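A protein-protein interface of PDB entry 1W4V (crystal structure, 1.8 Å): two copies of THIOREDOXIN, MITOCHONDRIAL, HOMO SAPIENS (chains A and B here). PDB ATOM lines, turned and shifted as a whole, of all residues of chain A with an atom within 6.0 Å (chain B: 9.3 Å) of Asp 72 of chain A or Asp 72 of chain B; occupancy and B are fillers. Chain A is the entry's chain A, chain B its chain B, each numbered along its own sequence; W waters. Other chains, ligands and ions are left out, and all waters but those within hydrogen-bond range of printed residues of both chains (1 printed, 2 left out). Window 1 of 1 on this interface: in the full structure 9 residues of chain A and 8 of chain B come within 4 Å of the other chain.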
ATOM      1  N   HIS A  39     -19.245  -7.508  10.840  1.00  0.00           N
ATOM      2  CA  HIS A  39     -19.467  -8.908  11.186  1.00  0.00           C
ATOM      3  C   HIS A  39     -19.009  -9.836  10.064  1.00  0.00           C
ATOM      4  O   HIS A  39     -18.746  -9.398   8.945  1.00  0.00           O
ATOM      5  CB  HIS A  39     -20.950  -9.144  11.502  1.00  0.00           C
ATOM      6  CG  HIS A  39     -21.850  -9.147  10.302  1.00  0.00           C
ATOM      7  ND1 HIS A  39     -22.189  -8.028   9.572  1.00  0.00           N
ATOM      8  CD2 HIS A  39     -22.420 -10.215   9.685  1.00  0.00           C
ATOM      9  CE1 HIS A  39     -22.886  -8.421   8.512  1.00  0.00           C
ATOM     10  NE2 HIS A  39     -23.079  -9.732   8.575  1.00  0.00           N
ATOM     11  N   ALA A  40     -19.003 -11.154  10.255  1.00  0.00           N
ATOM     12  CA  ALA A  40     -18.817 -12.151   9.195  1.00  0.00           C
ATOM     13  C   ALA A  40     -19.446 -13.449   9.671  1.00  0.00           C
ATOM     14  O   ALA A  40     -19.672 -13.603  10.877  1.00  0.00           O
ATOM     15  CB  ALA A  40     -17.313 -12.473   8.915  1.00  0.00           C
ATOM     16  N   GLN A  41     -19.710 -14.370   8.745  1.00  0.00           N
ATOM     17  CA  GLN A  41     -20.423 -15.613   8.963  1.00  0.00           C
ATOM     18  C   GLN A  41     -19.547 -16.493   9.873  1.00  0.00           C
ATOM     19  O   GLN A  41     -20.100 -17.386  10.533  1.00  0.00           O
ATOM     20  CB  GLN A  41     -20.727 -16.317   7.618  1.00  0.00           C
ATOM     21  CG  GLN A  41     -21.319 -15.648   6.365  1.00  0.00           C
ATOM     22  CD  GLN A  41     -20.957 -16.060   4.896  1.00  0.00           C
ATOM     23  OE1 GLN A  41     -20.798 -15.143   4.046  1.00  0.00           O
ATOM     24  NE2 GLN A  41     -20.886 -17.372   4.510  1.00  0.00           N
ATOM     25  N   TRP A  42     -18.222 -16.346   9.871  1.00  0.00           N
ATOM     26  CA  TRP A  42     -17.334 -17.174  10.673  1.00  0.00           C
ATOM     27  C   TRP A  42     -17.224 -16.707  12.134  1.00  0.00           C
ATOM     28  O   TRP A  42     -16.483 -17.300  12.906  1.00  0.00           O
ATOM     29  CB  TRP A  42     -15.943 -17.277  10.024  1.00  0.00           C
ATOM     30  CG  TRP A  42     -15.341 -15.974   9.496  1.00  0.00           C
ATOM     31  CD1 TRP A  42     -15.365 -15.616   8.180  1.00  0.00           C
ATOM     32  CD2 TRP A  42     -14.625 -14.928  10.158  1.00  0.00           C
ATOM     33  NE1 TRP A  42     -14.732 -14.409   7.982  1.00  0.00           N
ATOM     34  CE2 TRP A  42     -14.308 -13.956   9.204  1.00  0.00           C
ATOM     35  CE3 TRP A  42     -14.265 -14.668  11.492  1.00  0.00           C
ATOM     36  CZ2 TRP A  42     -13.573 -12.818   9.503  1.00  0.00           C
ATOM     37  CZ3 TRP A  42     -13.620 -13.482  11.793  1.00  0.00           C
ATOM     38  CH2 TRP A  42     -13.206 -12.601  10.800  1.00  0.00           C
ATOM     39  N   ASP A  70     -20.695  -6.802   6.182  1.00  0.00           N
ATOM     40  CA  ASP A  70     -20.051  -8.100   6.115  1.00  0.00           C
ATOM     41  C   ASP A  70     -18.640  -7.870   5.583  1.00  0.00           C
ATOM     42  O   ASP A  70     -18.422  -7.302   4.492  1.00  0.00           O
ATOM     43  CB  ASP A  70     -20.816  -9.087   5.232  1.00  0.00           C
ATOM     44  CG  ASP A  70     -20.130 -10.431   5.240  1.00  0.00           C
ATOM     45  OD1 ASP A  70     -18.995 -10.506   4.709  1.00  0.00           O
ATOM     46  OD2 ASP A  70     -20.641 -11.463   5.750  1.00  0.00           O
ATOM     47  N   ILE A  71     -17.675  -8.235   6.411  1.00  0.00           N
ATOM     48  CA  ILE A  71     -16.302  -7.824   6.157  1.00  0.00           C
ATOM     49  C   ILE A  71     -15.667  -8.754   5.154  1.00  0.00           C
ATOM     50  O   ILE A  71     -14.577  -8.474   4.685  1.00  0.00           O
ATOM     51  CB  ILE A  71     -15.459  -7.695   7.428  1.00  0.00           C
ATOM     52  CG1 ILE A  71     -15.277  -8.996   8.218  1.00  0.00           C
ATOM     53  CG2 ILE A  71     -15.975  -6.548   8.274  1.00  0.00           C
ATOM     54  CD1 ILE A  71     -14.100  -8.905   9.157  1.00  0.00           C
ATOM     55  N   ASP A  72     -16.279  -9.896   4.872  1.00  0.00           N
ATOM     56  CA  ASP A  72     -15.871 -10.724   3.783  1.00  0.00           C
ATOM     57  C   ASP A  72     -16.234 -10.073   2.441  1.00  0.00           C
ATOM     58  O   ASP A  72     -15.477 -10.062   1.455  1.00  0.00           O
ATOM     59  CB  ASP A  72     -16.452 -12.148   3.877  1.00  0.00           C
ATOM     60  CG  ASP A  72     -15.948 -12.913   5.073  1.00  0.00           C
ATOM     61  OD1 ASP A  72     -14.865 -12.593   5.627  1.00  0.00           O
ATOM     62  OD2 ASP A  72     -16.624 -13.910   5.402  1.00  0.00           O
ATOM     63  N   ASP A  73     -17.455  -9.547   2.375  1.00  0.00           N
ATOM     64  CA  ASP A  73     -17.979  -9.002   1.139  1.00  0.00           C
ATOM     65  C   ASP A  73     -17.423  -7.612   0.896  1.00  0.00           C
ATOM     66  O   ASP A  73     -17.427  -7.157  -0.252  1.00  0.00           O
ATOM     67  CB  ASP A  73     -19.510  -9.004   1.180  1.00  0.00           C
ATOM     68  CG  ASP A  73     -20.142 -10.378   1.337  1.00  0.00           C
ATOM     69  OD1 ASP A  73     -19.525 -11.389   0.923  1.00  0.00           O
ATOM     70  OD2 ASP A  73     -21.309 -10.463   1.768  1.00  0.00           O
ATOM     71  N   HIS A  74     -17.149  -6.917   1.994  1.00  0.00           N
ATOM     72  CA  HIS A  74     -16.700  -5.542   1.962  1.00  0.00           C
ATOM     73  C   HIS A  74     -15.455  -5.354   2.801  1.00  0.00           C
ATOM     74  O   HIS A  74     -15.383  -4.610   3.761  1.00  0.00           O
ATOM     75  CB  HIS A  74     -17.812  -4.609   2.422  1.00  0.00           C
ATOM     76  CG  HIS A  74     -19.111  -4.825   1.717  1.00  0.00           C
ATOM     77  ND1 HIS A  74     -19.368  -4.121   0.559  1.00  0.00           N
ATOM     78  CD2 HIS A  74     -20.103  -5.754   1.765  1.00  0.00           C
ATOM     79  CE1 HIS A  74     -20.537  -4.472   0.048  1.00  0.00           C
ATOM     80  NE2 HIS A  74     -21.004  -5.489   0.753  1.00  0.00           N
ATOM     81  N   THR A  75     -14.412  -6.078   2.410  1.00  0.00           N
ATOM     82  CA  THR A  75     -13.184  -5.949   3.164  1.00  0.00           C
ATOM     83  C   THR A  75     -12.568  -4.577   3.130  1.00  0.00           C
ATOM     84  O   THR A  75     -11.915  -4.182   4.083  1.00  0.00           O
ATOM     85  CB  THR A  75     -12.225  -6.964   2.541  1.00  0.00           C
ATOM     86  OG1 THR A  75     -12.891  -8.222   2.492  1.00  0.00           O
ATOM     87  CG2 THR A  75     -11.003  -7.153   3.421  1.00  0.00           C
ATOM     88  N   ILE B  17      -3.830 -20.402  -0.649  1.00  0.00           N
ATOM     89  CA  ILE B  17      -4.977 -21.218  -1.054  1.00  0.00           C
ATOM     90  C   ILE B  17      -5.980 -20.382  -1.830  1.00  0.00           C
ATOM     91  O   ILE B  17      -6.431 -19.310  -1.394  1.00  0.00           O
ATOM     92  CB  ILE B  17      -5.610 -21.743   0.247  1.00  0.00           C
ATOM     93  CG1 ILE B  17      -4.709 -22.751   0.945  1.00  0.00           C
ATOM     94  CG2 ILE B  17      -6.985 -22.343  -0.048  1.00  0.00           C
ATOM     95  CD1 ILE B  17      -4.373 -23.970   0.165  1.00  0.00           C
ATOM     96  N   ASP B  37      -2.377 -20.905   7.853  1.00  0.00           N
ATOM     97  CA  ASP B  37      -2.279 -19.545   8.379  1.00  0.00           C
ATOM     98  C   ASP B  37      -3.469 -18.774   7.860  1.00  0.00           C
ATOM     99  O   ASP B  37      -3.545 -18.334   6.700  1.00  0.00           O
ATOM    100  CB  ASP B  37      -0.936 -18.910   8.000  1.00  0.00           C
ATOM    101  CG  ASP B  37      -0.820 -17.464   8.332  1.00  0.00           C
ATOM    102  OD1 ASP B  37      -1.475 -16.974   9.263  1.00  0.00           O
ATOM    103  OD2 ASP B  37      -0.203 -16.702   7.567  1.00  0.00           O
ATOM    104  N   PHE B  38      -4.418 -18.550   8.765  1.00  0.00           N
ATOM    105  CA  PHE B  38      -5.605 -17.709   8.530  1.00  0.00           C
ATOM    106  C   PHE B  38      -5.299 -16.280   8.890  1.00  0.00           C
ATOM    107  O   PHE B  38      -4.983 -15.990  10.041  1.00  0.00           O
ATOM    108  CB  PHE B  38      -6.803 -18.147   9.372  1.00  0.00           C
ATOM    109  CG  PHE B  38      -7.437 -19.430   8.917  1.00  0.00           C
ATOM    110  CD1 PHE B  38      -6.916 -20.665   9.302  1.00  0.00           C
ATOM    111  CD2 PHE B  38      -8.548 -19.398   8.097  1.00  0.00           C
ATOM    112  CE1 PHE B  38      -7.467 -21.899   8.937  1.00  0.00           C
ATOM    113  CE2 PHE B  38      -9.092 -20.634   7.744  1.00  0.00           C
ATOM    114  CZ  PHE B  38      -8.565 -21.844   8.118  1.00  0.00           C
ATOM    115  N   HIS B  39      -5.305 -15.402   7.886  1.00  0.00           N
ATOM    116  CA  HIS B  39      -5.015 -13.983   8.021  1.00  0.00           C
ATOM    117  C   HIS B  39      -6.024 -13.081   7.304  1.00  0.00           C
ATOM    118  O   HIS B  39      -6.921 -13.548   6.601  1.00  0.00           O
ATOM    119  CB  HIS B  39      -3.596 -13.803   7.473  1.00  0.00           C
ATOM    120  CG  HIS B  39      -3.493 -13.939   5.987  1.00  0.00           C
ATOM    121  ND1 HIS B  39      -3.483 -15.146   5.314  1.00  0.00           N
ATOM    122  CD2 HIS B  39      -3.541 -12.970   5.051  1.00  0.00           C
ATOM    123  CE1 HIS B  39      -3.434 -14.903   4.015  1.00  0.00           C
ATOM    124  NE2 HIS B  39      -3.581 -13.606   3.836  1.00  0.00           N
ATOM    125  N   ALA B  40      -5.869 -11.766   7.442  1.00  0.00           N
ATOM    126  CA  ALA B  40      -6.754 -10.833   6.771  1.00  0.00           C
ATOM    127  C   ALA B  40      -5.990  -9.547   6.484  1.00  0.00           C
ATOM    128  O   ALA B  40      -5.046  -9.190   7.199  1.00  0.00           O
ATOM    129  CB  ALA B  40      -7.950 -10.540   7.668  1.00  0.00           C
ATOM    130  N   GLN B  41      -6.472  -8.807   5.487  1.00  0.00           N
ATOM    131  CA  GLN B  41      -5.775  -7.597   5.035  1.00  0.00           C
ATOM    132  C   GLN B  41      -5.851  -6.500   6.108  1.00  0.00           C
ATOM    133  O   GLN B  41      -4.967  -5.642   6.220  1.00  0.00           O
ATOM    134  CB  GLN B  41      -6.409  -7.099   3.736  1.00  0.00           C
ATOM    135  CG  GLN B  41      -6.315  -8.034   2.555  1.00  0.00           C
ATOM    136  CD  GLN B  41      -4.882  -8.410   2.230  1.00  0.00           C
ATOM    137  OE1 GLN B  41      -4.037  -7.516   2.117  1.00  0.00           O
ATOM    138  NE2 GLN B  41      -4.651  -9.721   2.077  1.00  0.00           N
ATOM    139  N   TRP B  42      -6.885  -6.535   6.951  1.00  0.00           N
ATOM    140  CA  TRP B  42      -7.110  -5.610   8.059  1.00  0.00           C
ATOM    141  C   TRP B  42      -6.399  -5.967   9.360  1.00  0.00           C
ATOM    142  O   TRP B  42      -6.417  -5.233  10.325  1.00  0.00           O
ATOM    143  CB  TRP B  42      -8.615  -5.436   8.323  1.00  0.00           C
ATOM    144  CG  TRP B  42      -9.418  -6.685   8.290  1.00  0.00           C
ATOM    145  CD1 TRP B  42     -10.205  -7.159   7.272  1.00  0.00           C
ATOM    146  CD2 TRP B  42      -9.550  -7.610   9.375  1.00  0.00           C
ATOM    147  NE1 TRP B  42     -10.790  -8.337   7.665  1.00  0.00           N
ATOM    148  CE2 TRP B  42     -10.467  -8.578   8.971  1.00  0.00           C
ATOM    149  CE3 TRP B  42      -9.034  -7.661  10.678  1.00  0.00           C
ATOM    150  CZ2 TRP B  42     -10.737  -9.673   9.760  1.00  0.00           C
ATOM    151  CZ3 TRP B  42      -9.376  -8.702  11.512  1.00  0.00           C
ATOM    152  CH2 TRP B  42     -10.235  -9.701  11.035  1.00  0.00           C
ATOM    153  N   CYS B  43      -5.637  -7.056   9.383  1.00  0.00           N
ATOM    154  CA  CYS B  43      -5.051  -7.553  10.619  1.00  0.00           C
ATOM    155  C   CYS B  43      -3.591  -7.112  10.701  1.00  0.00           C
ATOM    156  O   CYS B  43      -2.706  -7.589   9.994  1.00  0.00           O
ATOM    157  CB  CYS B  43      -5.177  -9.079  10.557  1.00  0.00           C
ATOM    158  SG  CYS B  43      -4.199 -10.074  11.736  1.00  0.00           S
ATOM    159  N   VAL B  69      -4.299 -18.665   4.090  1.00  0.00           N
ATOM    160  CA  VAL B  69      -5.732 -18.515   3.892  1.00  0.00           C
ATOM    161  C   VAL B  69      -6.205 -17.111   4.245  1.00  0.00           C
ATOM    162  O   VAL B  69      -6.229 -16.794   5.410  1.00  0.00           O
ATOM    163  CB  VAL B  69      -6.590 -19.544   4.637  1.00  0.00           C
ATOM    164  CG1 VAL B  69      -8.058 -19.488   4.308  1.00  0.00           C
ATOM    165  CG2 VAL B  69      -6.078 -20.963   4.334  1.00  0.00           C
ATOM    166  N   ASP B  70      -6.576 -16.332   3.239  1.00  0.00           N
ATOM    167  CA  ASP B  70      -7.146 -15.003   3.442  1.00  0.00           C
ATOM    168  C   ASP B  70      -8.581 -15.277   3.908  1.00  0.00           C
ATOM    169  O   ASP B  70      -9.346 -15.866   3.151  1.00  0.00           O
ATOM    170  CB  ASP B  70      -7.102 -14.098   2.233  1.00  0.00           C
ATOM    171  CG  ASP B  70      -7.585 -12.715   2.576  1.00  0.00           C
ATOM    172  OD1 ASP B  70      -8.608 -12.558   3.299  1.00  0.00           O
ATOM    173  OD2 ASP B  70      -6.980 -11.689   2.183  1.00  0.00           O
ATOM    174  N   ILE B  71      -8.865 -15.042   5.190  1.00  0.00           N
ATOM    175  CA  ILE B  71     -10.156 -15.411   5.804  1.00  0.00           C
ATOM    176  C   ILE B  71     -11.324 -14.847   4.985  1.00  0.00           C
ATOM    177  O   ILE B  71     -12.423 -15.429   4.892  1.00  0.00           O
ATOM    178  CB  ILE B  71     -10.227 -15.075   7.299  1.00  0.00           C
ATOM    179  CG1 ILE B  71     -11.309 -15.866   8.034  1.00  0.00           C
ATOM    180  CG2 ILE B  71     -10.231 -13.573   7.566  1.00  0.00           C
ATOM    181  CD1 ILE B  71     -11.136 -15.891   9.561  1.00  0.00           C
ATOM    182  N   ASP B  72     -11.108 -13.642   4.467  1.00  0.00           N
ATOM    183  CA  ASP B  72     -12.220 -12.914   3.865  1.00  0.00           C
ATOM    184  C   ASP B  72     -12.504 -13.469   2.471  1.00  0.00           C
ATOM    185  O   ASP B  72     -13.577 -13.189   1.929  1.00  0.00           O
ATOM    186  CB  ASP B  72     -12.004 -11.405   3.791  1.00  0.00           C
ATOM    187  CG  ASP B  72     -12.065 -10.775   5.133  1.00  0.00           C
ATOM    188  OD1 ASP B  72     -12.985 -11.089   5.911  1.00  0.00           O
ATOM    189  OD2 ASP B  72     -11.153 -10.023   5.506  1.00  0.00           O
ATOM    190  N   ASP B  73     -11.594 -14.274   1.920  1.00  0.00           N
ATOM    191  CA  ASP B  73     -11.802 -14.974   0.644  1.00  0.00           C
ATOM    192  C   ASP B  73     -12.160 -16.461   0.805  1.00  0.00           C
ATOM    193  O   ASP B  73     -12.330 -17.193  -0.169  1.00  0.00           O
ATOM    194  CB  ASP B  73     -10.564 -14.907  -0.246  1.00  0.00           C
ATOM    195  CG  ASP B  73     -10.010 -13.564  -0.694  1.00  0.00           C
ATOM    196  OD1 ASP B  73     -10.818 -12.716  -1.154  1.00  0.00           O
ATOM    197  OD2 ASP B  73      -8.776 -13.295  -0.808  1.00  0.00           O
ATOM    198  N   HIS B  74     -12.299 -16.922   2.058  1.00  0.00           N
ATOM    199  CA  HIS B  74     -12.473 -18.313   2.460  1.00  0.00           C
ATOM    200  C   HIS B  74     -13.368 -18.458   3.667  1.00  0.00           C
ATOM    201  O   HIS B  74     -13.050 -19.205   4.584  1.00  0.00           O
ATOM    202  CB  HIS B  74     -11.094 -18.936   2.680  1.00  0.00           C
ATOM    203  CG  HIS B  74     -10.326 -18.976   1.394  1.00  0.00           C
ATOM    204  ND1 HIS B  74     -10.566 -19.904   0.399  1.00  0.00           N
ATOM    205  CD2 HIS B  74      -9.406 -18.122   0.883  1.00  0.00           C
ATOM    206  CE1 HIS B  74      -9.890 -19.562  -0.686  1.00  0.00           C
ATOM    207  NE2 HIS B  74      -9.126 -18.527  -0.403  1.00  0.00           N
ATOM    208  N   THR B  75     -14.515 -17.779   3.614  1.00  0.00           N
ATOM    209  CA  THR B  75     -15.487 -17.915   4.666  1.00  0.00           C
ATOM    210  C   THR B  75     -15.738 -19.335   5.072  1.00  0.00           C
ATOM    211  O   THR B  75     -15.828 -19.682   6.261  1.00  0.00           O
ATOM    212  CB  THR B  75     -16.780 -17.248   4.171  1.00  0.00           C
ATOM    213  OG1 THR B  75     -16.519 -15.914   3.710  1.00  0.00           O
ATOM    214  CG2 THR B  75     -17.692 -17.192   5.394  1.00  0.00           C
ATOM    215  N   ASP B  76     -15.912 -20.163   4.040  1.00  0.00           N
ATOM    216  CA  ASP B  76     -16.107 -21.592   4.190  1.00  0.00           C
ATOM    217  C   ASP B  76     -15.112 -22.286   5.106  1.00  0.00           C
ATOM    218  O   ASP B  76     -15.509 -23.071   5.969  1.00  0.00           O
ATOM    219  CB  ASP B  76     -16.203 -22.234   2.816  1.00  0.00           C
ATOM    220  CG  ASP B  76     -14.956 -22.079   1.970  1.00  0.00           C
ATOM    221  OD1 ASP B  76     -14.160 -21.123   2.104  1.00  0.00           O
ATOM    222  OD2 ASP B  76     -14.720 -22.842   1.004  1.00  0.00           O
ATOM    223  N   LEU B  77     -13.834 -21.992   4.885  1.00  0.00           N
ATOM    224  CA  LEU B  77     -12.818 -22.740   5.616  1.00  0.00           C
ATOM    225  C   LEU B  77     -12.800 -22.201   7.021  1.00  0.00           C
ATOM    226  O   LEU B  77     -12.500 -22.954   7.928  1.00  0.00           O
ATOM    227  CB  LEU B  77     -11.432 -22.461   5.034  1.00  0.00           C
ATOM    228  CG  LEU B  77     -10.992 -23.332   3.851  1.00  0.00           C
ATOM    229  CD1 LEU B  77     -11.761 -24.616   3.558  1.00  0.00           C
ATOM    230  CD2 LEU B  77     -10.202 -22.641   2.778  1.00  0.00           C
ATOM    231  N   ALA B  78     -13.024 -20.905   7.215  1.00  0.00           N
ATOM    232  CA  ALA B  78     -13.052 -20.420   8.590  1.00  0.00           C
ATOM    233  C   ALA B  78     -14.233 -20.994   9.344  1.00  0.00           C
ATOM    234  O   ALA B  78     -14.168 -21.205  10.555  1.00  0.00           O
ATOM    235  CB  ALA B  78     -13.119 -18.918   8.623  1.00  0.00           C
ATOM    236  N   ILE B  79     -15.365 -21.123   8.654  1.00  0.00           N
ATOM    237  CA  ILE B  79     -16.504 -21.845   9.231  1.00  0.00           C
ATOM    238  C   ILE B  79     -16.085 -23.255   9.660  1.00  0.00           C
ATOM    239  O   ILE B  79     -16.371 -23.746  10.753  1.00  0.00           O
ATOM    240  CB  ILE B  79     -17.708 -21.716   8.243  1.00  0.00           C
ATOM    241  CG1 ILE B  79     -18.236 -20.276   8.220  1.00  0.00           C
ATOM    242  CG2 ILE B  79     -18.846 -22.644   8.655  1.00  0.00           C
ATOM    243  CD1 ILE B  79     -19.417 -20.107   7.293  1.00  0.00           C
ATOM    244  N   VAL B  83     -12.621 -20.863  12.947  1.00  0.00           N
ATOM    245  CA  VAL B  83     -11.690 -19.738  13.070  1.00  0.00           C
ATOM    246  C   VAL B  83     -12.529 -18.481  13.229  1.00  0.00           C
ATOM    247  O   VAL B  83     -13.283 -18.103  12.331  1.00  0.00           O
ATOM    248  CB  VAL B  83     -10.710 -19.632  11.895  1.00  0.00           C
ATOM    249  CG1 VAL B  83      -9.731 -18.440  11.975  1.00  0.00           C
ATOM    250  CG2 VAL B  83      -9.851 -20.891  11.774  1.00  0.00           C
ATOM    251  N   VAL B  86      -8.153 -13.657  13.683  1.00  0.00           N
ATOM    252  CA  VAL B  86      -6.849 -13.805  13.080  1.00  0.00           C
ATOM    253  C   VAL B  86      -5.796 -13.018  13.833  1.00  0.00           C
ATOM    254  O   VAL B  86      -6.114 -12.061  14.515  1.00  0.00           O
ATOM    255  CB  VAL B  86      -6.897 -13.311  11.619  1.00  0.00           C
ATOM    256  CG1 VAL B  86      -7.708 -14.308  10.776  1.00  0.00           C
ATOM    257  CG2 VAL B  86      -7.529 -11.922  11.483  1.00  0.00           C
HETATM  258  O   HOH W   1     -14.428 -11.511  -0.319  1.00  0.00           O
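The side-chain carboxylate of Asp 72 of chain B lies close to the side-chain carboxylate of Asp 72 of chain A (2.4 Å).
The side-chain hydroxyl (OG1) of Thr 75 of chain B sits at hydrogen-bond distance from the side-chain carboxylate (OD2) of Asp 72 of chain A.
The backbone carbonyl oxygen (O) of Val 83 of chain B sits close to the backbone carbonyl oxygen (O) of Trp 42 of chain A (3.3 Å).
The backbone carbonyl oxygen of Ile 71 of chain A lies close to the side-chain carboxylate of Asp 72 of chain B, at 3.3 Å.
The backbone carbonyl oxygen (O) of His 39 of chain A is in hydrogen-bond range of the backbone NH (N) of Ile 71 of chain A.
The indole nitrogen (NE1) of Trp 42 of chain A lies within hydrogen-bond range of the side-chain carboxylate (OD1) of Asp 72 of chain A, 3.0 Å away.
The backbone NH (N) of Asp 72 of chain A sits at hydrogen-bond distance from the side-chain carboxylate (OD1) of Asp 70 of chain A, 2.8 Å away.
The backbone carbonyl oxygen (O) of Asp 72 of chain A sits at hydrogen-bond distance from the side-chain hydroxyl (OG1) of Thr 75 of chain A (3.3 Å).
NE1 of Trp 42 of chain B is in hydrogen-bond range of OD2 of Asp 72 of chain B (2.8 Å).
The side-chain carboxylate (OD1) of Asp 70 of chain B is in hydrogen-bond range of the backbone NH (N) of Asp 72 of chain B.
Among the printed residues, merely in contact across the chains: Gln 41 of chain A with Thr 75 of chain B (3.3 Å), Trp 42 of chain A with Trp 42 of chain B (3.97 Å), Trp 42 of chain A with Ile 71 of chain B (3.7 Å), Trp 42 of chain A with Thr 75 of chain B (3.96 Å), Trp 42 of chain A with Ala 78 of chain B (3.6 Å), Ile 71 of chain A with Trp 42 of chain B (3.5 Å), Asp 72 of chain A with Ile 71 of chain B (3.8 Å), Thr 75 of chain A with Trp 42 of chain B (3.9 Å) and Thr 75 of chain A with Asp 72 of chain B (3.6 Å).
Printed residues of chain B within 4 Å of Gln 41 of chain A: Thr 75 (3.3 Å).
Ile 71 of chain A touches just these residues of chain B: Trp 42 (3.5 Å) and Asp 72 (3.3 Å).
Of chain B, only Ile 71 (3.8 Å), Asp 72 (2.4 Å) and Thr 75 (2.6 Å) come within 4 Å of Asp 72 of chain A.
No residue of chain B comes within 4 Å of Asp 73 of chain A.
Of the printed residues of chain B, Thr 75 of chain A touches Trp 42 (3.9 Å) and Asp 72 (3.6 Å).
Of the printed residues of chain A, Asp 72 of chain B touches Ile 71, Asp 72 and Thr 75.
Of the printed residues of chain A, Thr 75 of chain B touches Gln 41 (3.3 Å), Trp 42 (3.96 Å) and Asp 72 (2.6 Å).
The nearest residue of chain B that does not touch Asp 72 of chain A is Asp 73 of chain B (5.2 Å).
The nearest residue of chain A that does not touch Asp 72 of chain B is Trp 42 of chain A (4.03 Å).
The nearest printed residue of chain A that does not touch Ile 71 of chain B is Ile 71 of chain A (6.3 Å).
Of the 10 printed residues of chain A, 5 touch a printed residue of chain B.
Among the printed residues, 13 pairs touch across the chains.
Trp 42 of chain B touches its own counterpart, Trp 42 of chain A.
Trp 42 of chain A touches Ile 71 of chain B, and with the chains exchanged Ile 71 of chain A touches Trp 42 of chain B.
Trp 42 of chain A touches Thr 75 of chain B, and with the chains exchanged Thr 75 of chain A touches Trp 42 of chain B.
Asp 72 of chain B touches its own counterpart, Asp 72 of chain A.
Of the 13 pairs that touch across the chains among the printed residues, 10 have their exchanged pair printed and touching as well.
Water W1 lies within hydrogen-bond range of the backbone carbonyl oxygen (O) of Asp 72 of chain A and the backbone carbonyl oxygen (O) of Asp 72 of chain B.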
